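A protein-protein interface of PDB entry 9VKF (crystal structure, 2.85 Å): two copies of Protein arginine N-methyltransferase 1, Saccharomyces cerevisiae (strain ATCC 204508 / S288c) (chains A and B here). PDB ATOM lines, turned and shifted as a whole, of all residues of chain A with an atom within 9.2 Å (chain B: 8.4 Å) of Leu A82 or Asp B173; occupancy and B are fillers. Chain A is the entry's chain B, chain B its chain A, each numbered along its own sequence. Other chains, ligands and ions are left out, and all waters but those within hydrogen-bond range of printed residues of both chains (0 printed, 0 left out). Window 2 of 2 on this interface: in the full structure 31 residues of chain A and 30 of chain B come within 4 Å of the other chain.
Among the printed residues, merely in contact across the chains: Leu A82 with Asp B173, Ile A51 with Tyr B174, Ile A51 with Phe B172, Leu A79 with Tyr B174, Leu A82 with Pro B176, Phe A85 with Phe B172, Met A54 with Phe B172, Glu A78 with Pro B176, Asn A83 with Phe B172, Lys A58 with Phe B172, Leu A79 with Pro B176, Met A54 with Tyr B174, Met A75 with Phe B177 and Leu A79 with Asp B173.
Of the 16 printed residues of chain A, 10 touch a printed residue of chain B.
Printed residues of chain A that touch a printed residue of chain B: Thr A49, Ile A51, Met A54, Lys A58, Met A75, Glu A78, Leu A79, Leu A82, Asn A83 and Phe A85.
Hydrophobic or aromatic side chains of chain A within 4 Å of the printed part of chain B: Ile A51, Met A54, Met A75, Leu A79, Leu A82 and Phe A85.
Of the 14 printed residues of chain B, 5 touch a printed residue of chain A.
Among the printed residues, 17 pairs touch across the chains.
Among the printed residues, no Asp or Glu carboxylate lies within 4 Å of a Lys or Arg side-chain nitrogen of the other chain.
No position is printed for both chains.
The side-chain amide oxygen (OD1) of Asn A83 sits at hydrogen-bond distance from the backbone NH (N) of Asp B173.
The side-chain sulfur (SD) of Met A75 lies close to the backbone carbonyl oxygen (O) of Pro B176.
The side-chain hydroxyl of Tyr B174 lies within hydrogen-bond range of the side-chain hydroxyl of Thr A49, 3.0 Å away.
Of the printed residues of chain B, Leu A82 touches Asp B173 (3.3 Å) and Pro B176 (3.6 Å).
Of the printed residues of chain B, Asn A83 touches Phe B172 (3.7 Å) and Asp B173 (3.0 Å).
Of the printed residues of chain B, Glu A78 touches Pro B176 (3.7 Å).
Of the printed residues of chain B, Ile A51 touches Phe B172 and Tyr B174.
Printed residues of chain B within 4 Å of Lys A58: Phe B172 (3.7 Å).
The nearest residue of chain A that does not touch Asp B173 is Met A54 (6.0 Å).
The backbone carbonyl oxygen (O) of Val A80 lies within hydrogen-bond range of the backbone NH (N) of Phe A85 (3.0 Å).
The side-chain amide nitrogen (ND2) of Asn A83 sits at hydrogen-bond distance from the backbone carbonyl oxygen (O) of Leu A79 (3.0 Å).
The backbone NH (N) of Tyr B174 sits close to the backbone carbonyl oxygen (O) of Trp B166 (3.1 Å).
The side-chain hydroxyl of Ser B175 is in hydrogen-bond range of the side-chain carboxylate of Asp B173, at 2.8 Å.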
ATOM      1  N   THR A  49      21.378  16.102  27.329  1.00  0.00           N
ATOM      2  CA  THR A  49      20.645  17.051  26.502  1.00  0.00           C
ATOM      3  C   THR A  49      21.522  17.712  25.445  1.00  0.00           C
ATOM      4  O   THR A  49      20.986  18.394  24.564  1.00  0.00           O
ATOM      5  CB  THR A  49      20.000  18.131  27.376  1.00  0.00           C
ATOM      6  OG1 THR A  49      21.011  18.815  28.126  1.00  0.00           O
ATOM      7  CG2 THR A  49      18.999  17.513  28.336  1.00  0.00           C
ATOM      8  N   ILE A  51      24.165  19.910  26.112  1.00  0.00           N
ATOM      9  CA  ILE A  51      24.571  21.266  26.477  1.00  0.00           C
ATOM     10  C   ILE A  51      26.066  21.467  26.254  1.00  0.00           C
ATOM     11  O   ILE A  51      26.500  22.526  25.783  1.00  0.00           O
ATOM     12  CB  ILE A  51      24.164  21.564  27.934  1.00  0.00           C
ATOM     13  CG1 ILE A  51      24.668  22.940  28.375  1.00  0.00           C
ATOM     14  CG2 ILE A  51      24.660  20.470  28.871  1.00  0.00           C
ATOM     15  CD1 ILE A  51      23.844  24.091  27.854  1.00  0.00           C
ATOM     16  N   MET A  54      26.776  21.768  22.427  1.00  0.00           N
ATOM     17  CA  MET A  54      26.446  23.095  21.920  1.00  0.00           C
ATOM     18  C   MET A  54      27.474  24.132  22.353  1.00  0.00           C
ATOM     19  O   MET A  54      27.763  25.069  21.600  1.00  0.00           O
ATOM     20  CB  MET A  54      25.044  23.500  22.382  1.00  0.00           C
ATOM     21  CG  MET A  54      23.942  22.560  21.909  1.00  0.00           C
ATOM     22  SD  MET A  54      22.305  23.316  21.931  1.00  0.00           S
ATOM     23  CE  MET A  54      21.698  22.760  23.522  1.00  0.00           C
ATOM     24  N   LYS A  58      29.511  26.211  19.439  1.00  0.00           N
ATOM     25  CA  LYS A  58      29.380  27.662  19.337  1.00  0.00           C
ATOM     26  C   LYS A  58      30.723  28.366  19.481  1.00  0.00           C
ATOM     27  O   LYS A  58      30.901  29.469  18.951  1.00  0.00           O
ATOM     28  CB  LYS A  58      28.380  28.190  20.370  1.00  0.00           C
ATOM     29  CG  LYS A  58      28.907  28.293  21.790  1.00  0.00           C
ATOM     30  CD  LYS A  58      27.869  28.905  22.720  1.00  0.00           C
ATOM     31  CE  LYS A  58      27.462  30.300  22.265  1.00  0.00           C
ATOM     32  NZ  LYS A  58      26.544  30.959  23.241  1.00  0.00           N
ATOM     33  N   MET A  75      15.442  14.463  22.302  1.00  0.00           N
ATOM     34  CA  MET A  75      15.344  15.854  22.730  1.00  0.00           C
ATOM     35  C   MET A  75      16.586  16.640  22.332  1.00  0.00           C
ATOM     36  O   MET A  75      16.485  17.801  21.915  1.00  0.00           O
ATOM     37  CB  MET A  75      15.119  15.923  24.240  1.00  0.00           C
ATOM     38  CG  MET A  75      14.875  17.328  24.765  1.00  0.00           C
ATOM     39  SD  MET A  75      13.379  18.069  24.100  1.00  0.00           S
ATOM     40  CE  MET A  75      12.190  16.758  24.400  1.00  0.00           C
ATOM     41  N   ALA A  76      17.766  16.030  22.473  1.00  0.00           N
ATOM     42  CA  ALA A  76      19.004  16.701  22.089  1.00  0.00           C
ATOM     43  C   ALA A  76      18.987  17.117  20.621  1.00  0.00           C
ATOM     44  O   ALA A  76      19.382  18.240  20.286  1.00  0.00           O
ATOM     45  CB  ALA A  76      20.202  15.797  22.379  1.00  0.00           C
ATOM     46  N   LYS A  77      18.544  16.224  19.729  1.00  0.00           N
ATOM     47  CA  LYS A  77      18.432  16.591  18.320  1.00  0.00           C
ATOM     48  C   LYS A  77      17.514  17.793  18.132  1.00  0.00           C
ATOM     49  O   LYS A  77      17.800  18.682  17.321  1.00  0.00           O
ATOM     50  CB  LYS A  77      17.942  15.401  17.493  1.00  0.00           C
ATOM     51  CG  LYS A  77      18.905  14.227  17.459  1.00  0.00           C
ATOM     52  CD  LYS A  77      18.369  13.100  16.594  1.00  0.00           C
ATOM     53  CE  LYS A  77      19.469  12.115  16.236  1.00  0.00           C
ATOM     54  NZ  LYS A  77      19.013  11.087  15.264  1.00  0.00           N
ATOM     55  N   GLU A  78      16.401  17.832  18.868  1.00  0.00           N
ATOM     56  CA  GLU A  78      15.476  18.954  18.753  1.00  0.00           C
ATOM     57  C   GLU A  78      16.098  20.241  19.286  1.00  0.00           C
ATOM     58  O   GLU A  78      15.934  21.310  18.686  1.00  0.00           O
ATOM     59  CB  GLU A  78      14.174  18.634  19.488  1.00  0.00           C
ATOM     60  CG  GLU A  78      13.007  19.539  19.117  1.00  0.00           C
ATOM     61  CD  GLU A  78      11.680  19.038  19.660  1.00  0.00           C
ATOM     62  OE1 GLU A  78      11.643  17.923  20.221  1.00  0.00           O
ATOM     63  OE2 GLU A  78      10.673  19.762  19.522  1.00  0.00           O
ATOM     64  N   LEU A  79      16.812  20.160  20.410  1.00  0.00           N
ATOM     65  CA  LEU A  79      17.474  21.340  20.961  1.00  0.00           C
ATOM     66  C   LEU A  79      18.586  21.829  20.042  1.00  0.00           C
ATOM     67  O   LEU A  79      18.714  23.033  19.791  1.00  0.00           O
ATOM     68  CB  LEU A  79      18.026  21.033  22.352  1.00  0.00           C
ATOM     69  CG  LEU A  79      17.018  20.646  23.433  1.00  0.00           C
ATOM     70  CD1 LEU A  79      17.746  20.138  24.664  1.00  0.00           C
ATOM     71  CD2 LEU A  79      16.129  21.826  23.785  1.00  0.00           C
ATOM     72  N   VAL A  80      19.408  20.905  19.539  1.00  0.00           N
ATOM     73  CA  VAL A  80      20.476  21.279  18.616  1.00  0.00           C
ATOM     74  C   VAL A  80      19.893  21.917  17.360  1.00  0.00           C
ATOM     75  O   VAL A  80      20.447  22.884  16.821  1.00  0.00           O
ATOM     76  CB  VAL A  80      21.347  20.051  18.287  1.00  0.00           C
ATOM     77  CG1 VAL A  80      22.274  20.345  17.123  1.00  0.00           C
ATOM     78  CG2 VAL A  80      22.150  19.627  19.511  1.00  0.00           C
ATOM     79  N   GLU A  81      18.762  21.396  16.883  1.00  0.00           N
ATOM     80  CA  GLU A  81      18.099  21.996  15.730  1.00  0.00           C
ATOM     81  C   GLU A  81      17.602  23.404  16.038  1.00  0.00           C
ATOM     82  O   GLU A  81      17.719  24.308  15.203  1.00  0.00           O
ATOM     83  CB  GLU A  81      16.939  21.111  15.273  1.00  0.00           C
ATOM     84  CG  GLU A  81      16.089  21.722  14.170  1.00  0.00           C
ATOM     85  CD  GLU A  81      16.844  21.869  12.864  1.00  0.00           C
ATOM     86  OE1 GLU A  81      17.717  21.021  12.581  1.00  0.00           O
ATOM     87  OE2 GLU A  81      16.568  22.836  12.125  1.00  0.00           O
ATOM     88  N   LEU A  82      17.044  23.608  17.233  1.00  0.00           N
ATOM     89  CA  LEU A  82      16.404  24.883  17.539  1.00  0.00           C
ATOM     90  C   LEU A  82      17.418  26.003  17.735  1.00  0.00           C
ATOM     91  O   LEU A  82      17.101  27.173  17.489  1.00  0.00           O
ATOM     92  CB  LEU A  82      15.521  24.732  18.779  1.00  0.00           C
ATOM     93  CG  LEU A  82      14.753  25.967  19.251  1.00  0.00           C
ATOM     94  CD1 LEU A  82      13.702  26.362  18.227  1.00  0.00           C
ATOM     95  CD2 LEU A  82      14.110  25.704  20.597  1.00  0.00           C
ATOM     96  N   ASN A  83      18.636  25.677  18.162  1.00  0.00           N
ATOM     97  CA  ASN A  83      19.658  26.683  18.416  1.00  0.00           C
ATOM     98  C   ASN A  83      20.657  26.813  17.271  1.00  0.00           C
ATOM     99  O   ASN A  83      21.712  27.429  17.451  1.00  0.00           O
ATOM    100  CB  ASN A  83      20.388  26.378  19.725  1.00  0.00           C
ATOM    101  CG  ASN A  83      19.497  26.554  20.941  1.00  0.00           C
ATOM    102  OD1 ASN A  83      19.176  27.677  21.334  1.00  0.00           O
ATOM    103  ND2 ASN A  83      19.088  25.443  21.542  1.00  0.00           N
ATOM    104  N   GLY A  84      20.351  26.251  16.104  1.00  0.00           N
ATOM    105  CA  GLY A  84      21.163  26.480  14.925  1.00  0.00           C
ATOM    106  C   GLY A  84      22.490  25.756  14.882  1.00  0.00           C
ATOM    107  O   GLY A  84      23.453  26.284  14.319  1.00  0.00           O
ATOM    108  N   PHE A  85      22.573  24.555  15.460  1.00  0.00           N
ATOM    109  CA  PHE A  85      23.815  23.789  15.480  1.00  0.00           C
ATOM    110  C   PHE A  85      23.676  22.454  14.755  1.00  0.00           C
ATOM    111  O   PHE A  85      24.504  21.558  14.951  1.00  0.00           O
ATOM    112  CB  PHE A  85      24.280  23.556  16.918  1.00  0.00           C
ATOM    113  CG  PHE A  85      24.645  24.813  17.649  1.00  0.00           C
ATOM    114  CD1 PHE A  85      25.762  25.547  17.283  1.00  0.00           C
ATOM    115  CD2 PHE A  85      23.869  25.264  18.704  1.00  0.00           C
ATOM    116  CE1 PHE A  85      26.099  26.707  17.958  1.00  0.00           C
ATOM    117  CE2 PHE A  85      24.199  26.424  19.382  1.00  0.00           C
ATOM    118  CZ  PHE A  85      25.314  27.145  19.006  1.00  0.00           C
ATOM    119  N   SER A  86      22.643  22.302  13.924  1.00  0.00           N
ATOM    120  CA  SER A  86      22.399  21.020  13.269  1.00  0.00           C
ATOM    121  C   SER A  86      23.501  20.660  12.279  1.00  0.00           C
ATOM    122  O   SER A  86      23.758  19.473  12.049  1.00  0.00           O
ATOM    123  CB  SER A  86      21.038  21.037  12.572  1.00  0.00           C
ATOM    124  OG  SER A  86      20.936  22.134  11.682  1.00  0.00           O
ATOM    125  N   TYR B 165      12.177  27.828  33.656  1.00  0.00           N
ATOM    126  CA  TYR B 165      13.579  27.561  33.627  1.00  0.00           C
ATOM    127  C   TYR B 165      14.038  27.238  32.265  1.00  0.00           C
ATOM    128  O   TYR B 165      15.165  27.534  31.918  1.00  0.00           O
ATOM    129  CB  TYR B 165      13.868  26.342  34.462  1.00  0.00           C
ATOM    130  CG  TYR B 165      15.313  25.932  34.462  1.00  0.00           C
ATOM    131  CD1 TYR B 165      16.227  26.560  35.280  1.00  0.00           C
ATOM    132  CD2 TYR B 165      15.761  24.918  33.644  1.00  0.00           C
ATOM    133  CE1 TYR B 165      17.552  26.191  35.283  1.00  0.00           C
ATOM    134  CE2 TYR B 165      17.084  24.541  33.640  1.00  0.00           C
ATOM    135  CZ  TYR B 165      17.972  25.186  34.463  1.00  0.00           C
ATOM    136  OH  TYR B 165      19.287  24.819  34.470  1.00  0.00           O
ATOM    137  N   TRP B 166      13.163  26.675  31.455  1.00  0.00           N
ATOM    138  CA  TRP B 166      13.607  26.169  30.164  1.00  0.00           C
ATOM    139  C   TRP B 166      13.528  27.198  29.044  1.00  0.00           C
ATOM    140  O   TRP B 166      13.908  26.887  27.912  1.00  0.00           O
ATOM    141  CB  TRP B 166      12.797  24.928  29.794  1.00  0.00           C
ATOM    142  CG  TRP B 166      12.828  23.903  30.878  1.00  0.00           C
ATOM    143  CD1 TRP B 166      11.830  23.609  31.758  1.00  0.00           C
ATOM    144  CD2 TRP B 166      13.932  23.061  31.225  1.00  0.00           C
ATOM    145  NE1 TRP B 166      12.237  22.621  32.621  1.00  0.00           N
ATOM    146  CE2 TRP B 166      13.525  22.268  32.315  1.00  0.00           C
ATOM    147  CE3 TRP B 166      15.222  22.893  30.712  1.00  0.00           C
ATOM    148  CZ2 TRP B 166      14.362  21.322  32.902  1.00  0.00           C
ATOM    149  CZ3 TRP B 166      16.050  21.954  31.296  1.00  0.00           C
ATOM    150  CH2 TRP B 166      15.618  21.181  32.379  1.00  0.00           C
ATOM    151  N   GLN B 167      13.049  28.410  29.323  1.00  0.00           N
ATOM    152  CA  GLN B 167      13.041  29.436  28.287  1.00  0.00           C
ATOM    153  C   GLN B 167      14.452  29.889  27.936  1.00  0.00           C
ATOM    154  O   GLN B 167      14.713  30.259  26.786  1.00  0.00           O
ATOM    155  CB  GLN B 167      12.197  30.627  28.731  1.00  0.00           C
ATOM    156  CG  GLN B 167      10.707  30.342  28.758  1.00  0.00           C
ATOM    157  CD  GLN B 167      10.186  29.842  27.424  1.00  0.00           C
ATOM    158  OE1 GLN B 167      10.183  30.572  26.432  1.00  0.00           O
ATOM    159  NE2 GLN B 167       9.747  28.591  27.393  1.00  0.00           N
ATOM    160  N   ASP B 168      15.368  29.868  28.905  1.00  0.00           N
ATOM    161  CA  ASP B 168      16.730  30.355  28.692  1.00  0.00           C
ATOM    162  C   ASP B 168      17.649  29.576  29.631  1.00  0.00           C
ATOM    163  O   ASP B 168      17.680  29.845  30.835  1.00  0.00           O
ATOM    164  CB  ASP B 168      16.812  31.856  28.937  1.00  0.00           C
ATOM    165  CG  ASP B 168      18.086  32.469  28.399  1.00  0.00           C
ATOM    166  OD1 ASP B 168      19.094  31.744  28.292  1.00  0.00           O
ATOM    167  OD2 ASP B 168      18.078  33.675  28.073  1.00  0.00           O
ATOM    168  N   VAL B 169      18.388  28.620  29.074  1.00  0.00           N
ATOM    169  CA  VAL B 169      19.298  27.770  29.836  1.00  0.00           C
ATOM    170  C   VAL B 169      20.709  28.070  29.343  1.00  0.00           C
ATOM    171  O   VAL B 169      21.142  27.540  28.312  1.00  0.00           O
ATOM    172  CB  VAL B 169      18.961  26.283  29.693  1.00  0.00           C
ATOM    173  CG1 VAL B 169      19.982  25.430  30.432  1.00  0.00           C
ATOM    174  CG2 VAL B 169      17.562  26.008  30.217  1.00  0.00           C
ATOM    175  N   TYR B 170      21.427  28.923  30.079  1.00  0.00           N
ATOM    176  CA  TYR B 170      22.785  29.340  29.718  1.00  0.00           C
ATOM    177  C   TYR B 170      22.829  29.953  28.319  1.00  0.00           C
ATOM    178  O   TYR B 170      23.794  29.776  27.574  1.00  0.00           O
ATOM    179  CB  TYR B 170      23.773  28.177  29.832  1.00  0.00           C
ATOM    180  CG  TYR B 170      23.861  27.570  31.214  1.00  0.00           C
ATOM    181  CD1 TYR B 170      24.589  28.190  32.221  1.00  0.00           C
ATOM    182  CD2 TYR B 170      23.224  26.371  31.511  1.00  0.00           C
ATOM    183  CE1 TYR B 170      24.676  27.640  33.486  1.00  0.00           C
ATOM    184  CE2 TYR B 170      23.304  25.812  32.775  1.00  0.00           C
ATOM    185  CZ  TYR B 170      24.033  26.450  33.757  1.00  0.00           C
ATOM    186  OH  TYR B 170      24.118  25.899  35.013  1.00  0.00           O
ATOM    187  N   GLY B 171      21.774  30.689  27.962  1.00  0.00           N
ATOM    188  CA  GLY B 171      21.653  31.325  26.674  1.00  0.00           C
ATOM    189  C   GLY B 171      20.847  30.529  25.665  1.00  0.00           C
ATOM    190  O   GLY B 171      20.251  31.120  24.758  1.00  0.00           O
ATOM    191  N   PHE B 172      20.805  29.208  25.812  1.00  0.00           N
ATOM    192  CA  PHE B 172      20.163  28.351  24.825  1.00  0.00           C
ATOM    193  C   PHE B 172      18.665  28.246  25.073  1.00  0.00           C
ATOM    194  O   PHE B 172      18.209  28.194  26.221  1.00  0.00           O
ATOM    195  CB  PHE B 172      20.792  26.960  24.844  1.00  0.00           C
ATOM    196  CG  PHE B 172      22.230  26.945  24.422  1.00  0.00           C
ATOM    197  CD1 PHE B 172      22.610  27.460  23.195  1.00  0.00           C
ATOM    198  CD2 PHE B 172      23.202  26.418  25.253  1.00  0.00           C
ATOM    199  CE1 PHE B 172      23.932  27.449  22.804  1.00  0.00           C
ATOM    200  CE2 PHE B 172      24.526  26.403  24.869  1.00  0.00           C
ATOM    201  CZ  PHE B 172      24.893  26.920  23.642  1.00  0.00           C
ATOM    202  N   ASP B 173      17.902  28.215  23.982  1.00  0.00           N
ATOM    203  CA  ASP B 173      16.461  28.005  24.044  1.00  0.00           C
ATOM    204  C   ASP B 173      16.189  26.527  24.302  1.00  0.00           C
ATOM    205  O   ASP B 173      16.406  25.685  23.424  1.00  0.00           O
ATOM    206  CB  ASP B 173      15.802  28.472  22.749  1.00  0.00           C
ATOM    207  CG  ASP B 173      14.288  28.469  22.829  1.00  0.00           C
ATOM    208  OD1 ASP B 173      13.744  28.247  23.931  1.00  0.00           O
ATOM    209  OD2 ASP B 173      13.641  28.699  21.785  1.00  0.00           O
ATOM    210  N   TYR B 174      15.711  26.210  25.507  1.00  0.00           N
ATOM    211  CA  TYR B 174      15.321  24.855  25.878  1.00  0.00           C
ATOM    212  C   TYR B 174      13.807  24.675  25.872  1.00  0.00           C
ATOM    213  O   TYR B 174      13.265  23.927  26.692  1.00  0.00           O
ATOM    214  CB  TYR B 174      15.894  24.496  27.250  1.00  0.00           C
ATOM    215  CG  TYR B 174      17.194  23.725  27.208  1.00  0.00           C
ATOM    216  CD1 TYR B 174      18.326  24.258  26.603  1.00  0.00           C
ATOM    217  CD2 TYR B 174      17.290  22.466  27.783  1.00  0.00           C
ATOM    218  CE1 TYR B 174      19.518  23.552  26.569  1.00  0.00           C
ATOM    219  CE2 TYR B 174      18.474  21.753  27.756  1.00  0.00           C
ATOM    220  CZ  TYR B 174      19.585  22.299  27.147  1.00  0.00           C
ATOM    221  OH  TYR B 174      20.766  21.591  27.118  1.00  0.00           O
ATOM    222  N   SER B 175      13.116  25.364  24.963  1.00  0.00           N
ATOM    223  CA  SER B 175      11.657  25.291  24.914  1.00  0.00           C
ATOM    224  C   SER B 175      11.103  23.883  24.714  1.00  0.00           C
ATOM    225  O   SER B 175      10.134  23.536  25.412  1.00  0.00           O
ATOM    226  CB  SER B 175      11.136  26.233  23.820  1.00  0.00           C
ATOM    227  OG  SER B 175      11.079  27.571  24.282  1.00  0.00           O
ATOM    228  N   PRO B 176      11.661  23.113  23.813  1.00  0.00           N
ATOM    229  CA  PRO B 176      11.060  21.808  23.582  1.00  0.00           C
ATOM    230  C   PRO B 176      10.966  20.937  24.813  1.00  0.00           C
ATOM    231  O   PRO B 176      10.290  19.929  24.749  1.00  0.00           O
ATOM    232  CB  PRO B 176      12.044  21.173  22.614  1.00  0.00           C
ATOM    233  CG  PRO B 176      12.713  22.294  21.924  1.00  0.00           C
ATOM    234  CD  PRO B 176      12.843  23.343  22.970  1.00  0.00           C
ATOM    235  N   PHE B 177      11.643  21.277  25.891  1.00  0.00           N
ATOM    236  CA  PHE B 177      11.708  20.432  27.064  1.00  0.00           C
ATOM    237  C   PHE B 177      10.541  20.558  27.966  1.00  0.00           C
ATOM    238  O   PHE B 177      10.185  19.649  28.677  1.00  0.00           O
ATOM    239  CB  PHE B 177      12.928  20.846  27.855  1.00  0.00           C
ATOM    240  CG  PHE B 177      13.474  19.787  28.746  1.00  0.00           C
ATOM    241  CD1 PHE B 177      14.369  18.861  28.268  1.00  0.00           C
ATOM    242  CD2 PHE B 177      13.119  19.747  30.070  1.00  0.00           C
ATOM    243  CE1 PHE B 177      14.885  17.892  29.094  1.00  0.00           C
ATOM    244  CE2 PHE B 177      13.629  18.786  30.904  1.00  0.00           C
ATOM    245  CZ  PHE B 177      14.517  17.855  30.416  1.00  0.00           C
ATOM    246  N   VAL B 178       9.834  21.665  27.900  1.00  0.00           N
ATOM    247  CA  VAL B 178       8.724  21.882  28.815  1.00  0.00           C
ATOM    248  C   VAL B 178       7.673  20.800  28.762  1.00  0.00           C
ATOM    249  O   VAL B 178       7.223  20.353  29.791  1.00  0.00           O
ATOM    250  CB  VAL B 178       8.038  23.228  28.560  1.00  0.00           C
ATOM    251  CG1 VAL B 178       6.613  23.201  29.079  1.00  0.00           C
ATOM    252  CG2 VAL B 178       8.807  24.323  29.269  1.00  0.00           C
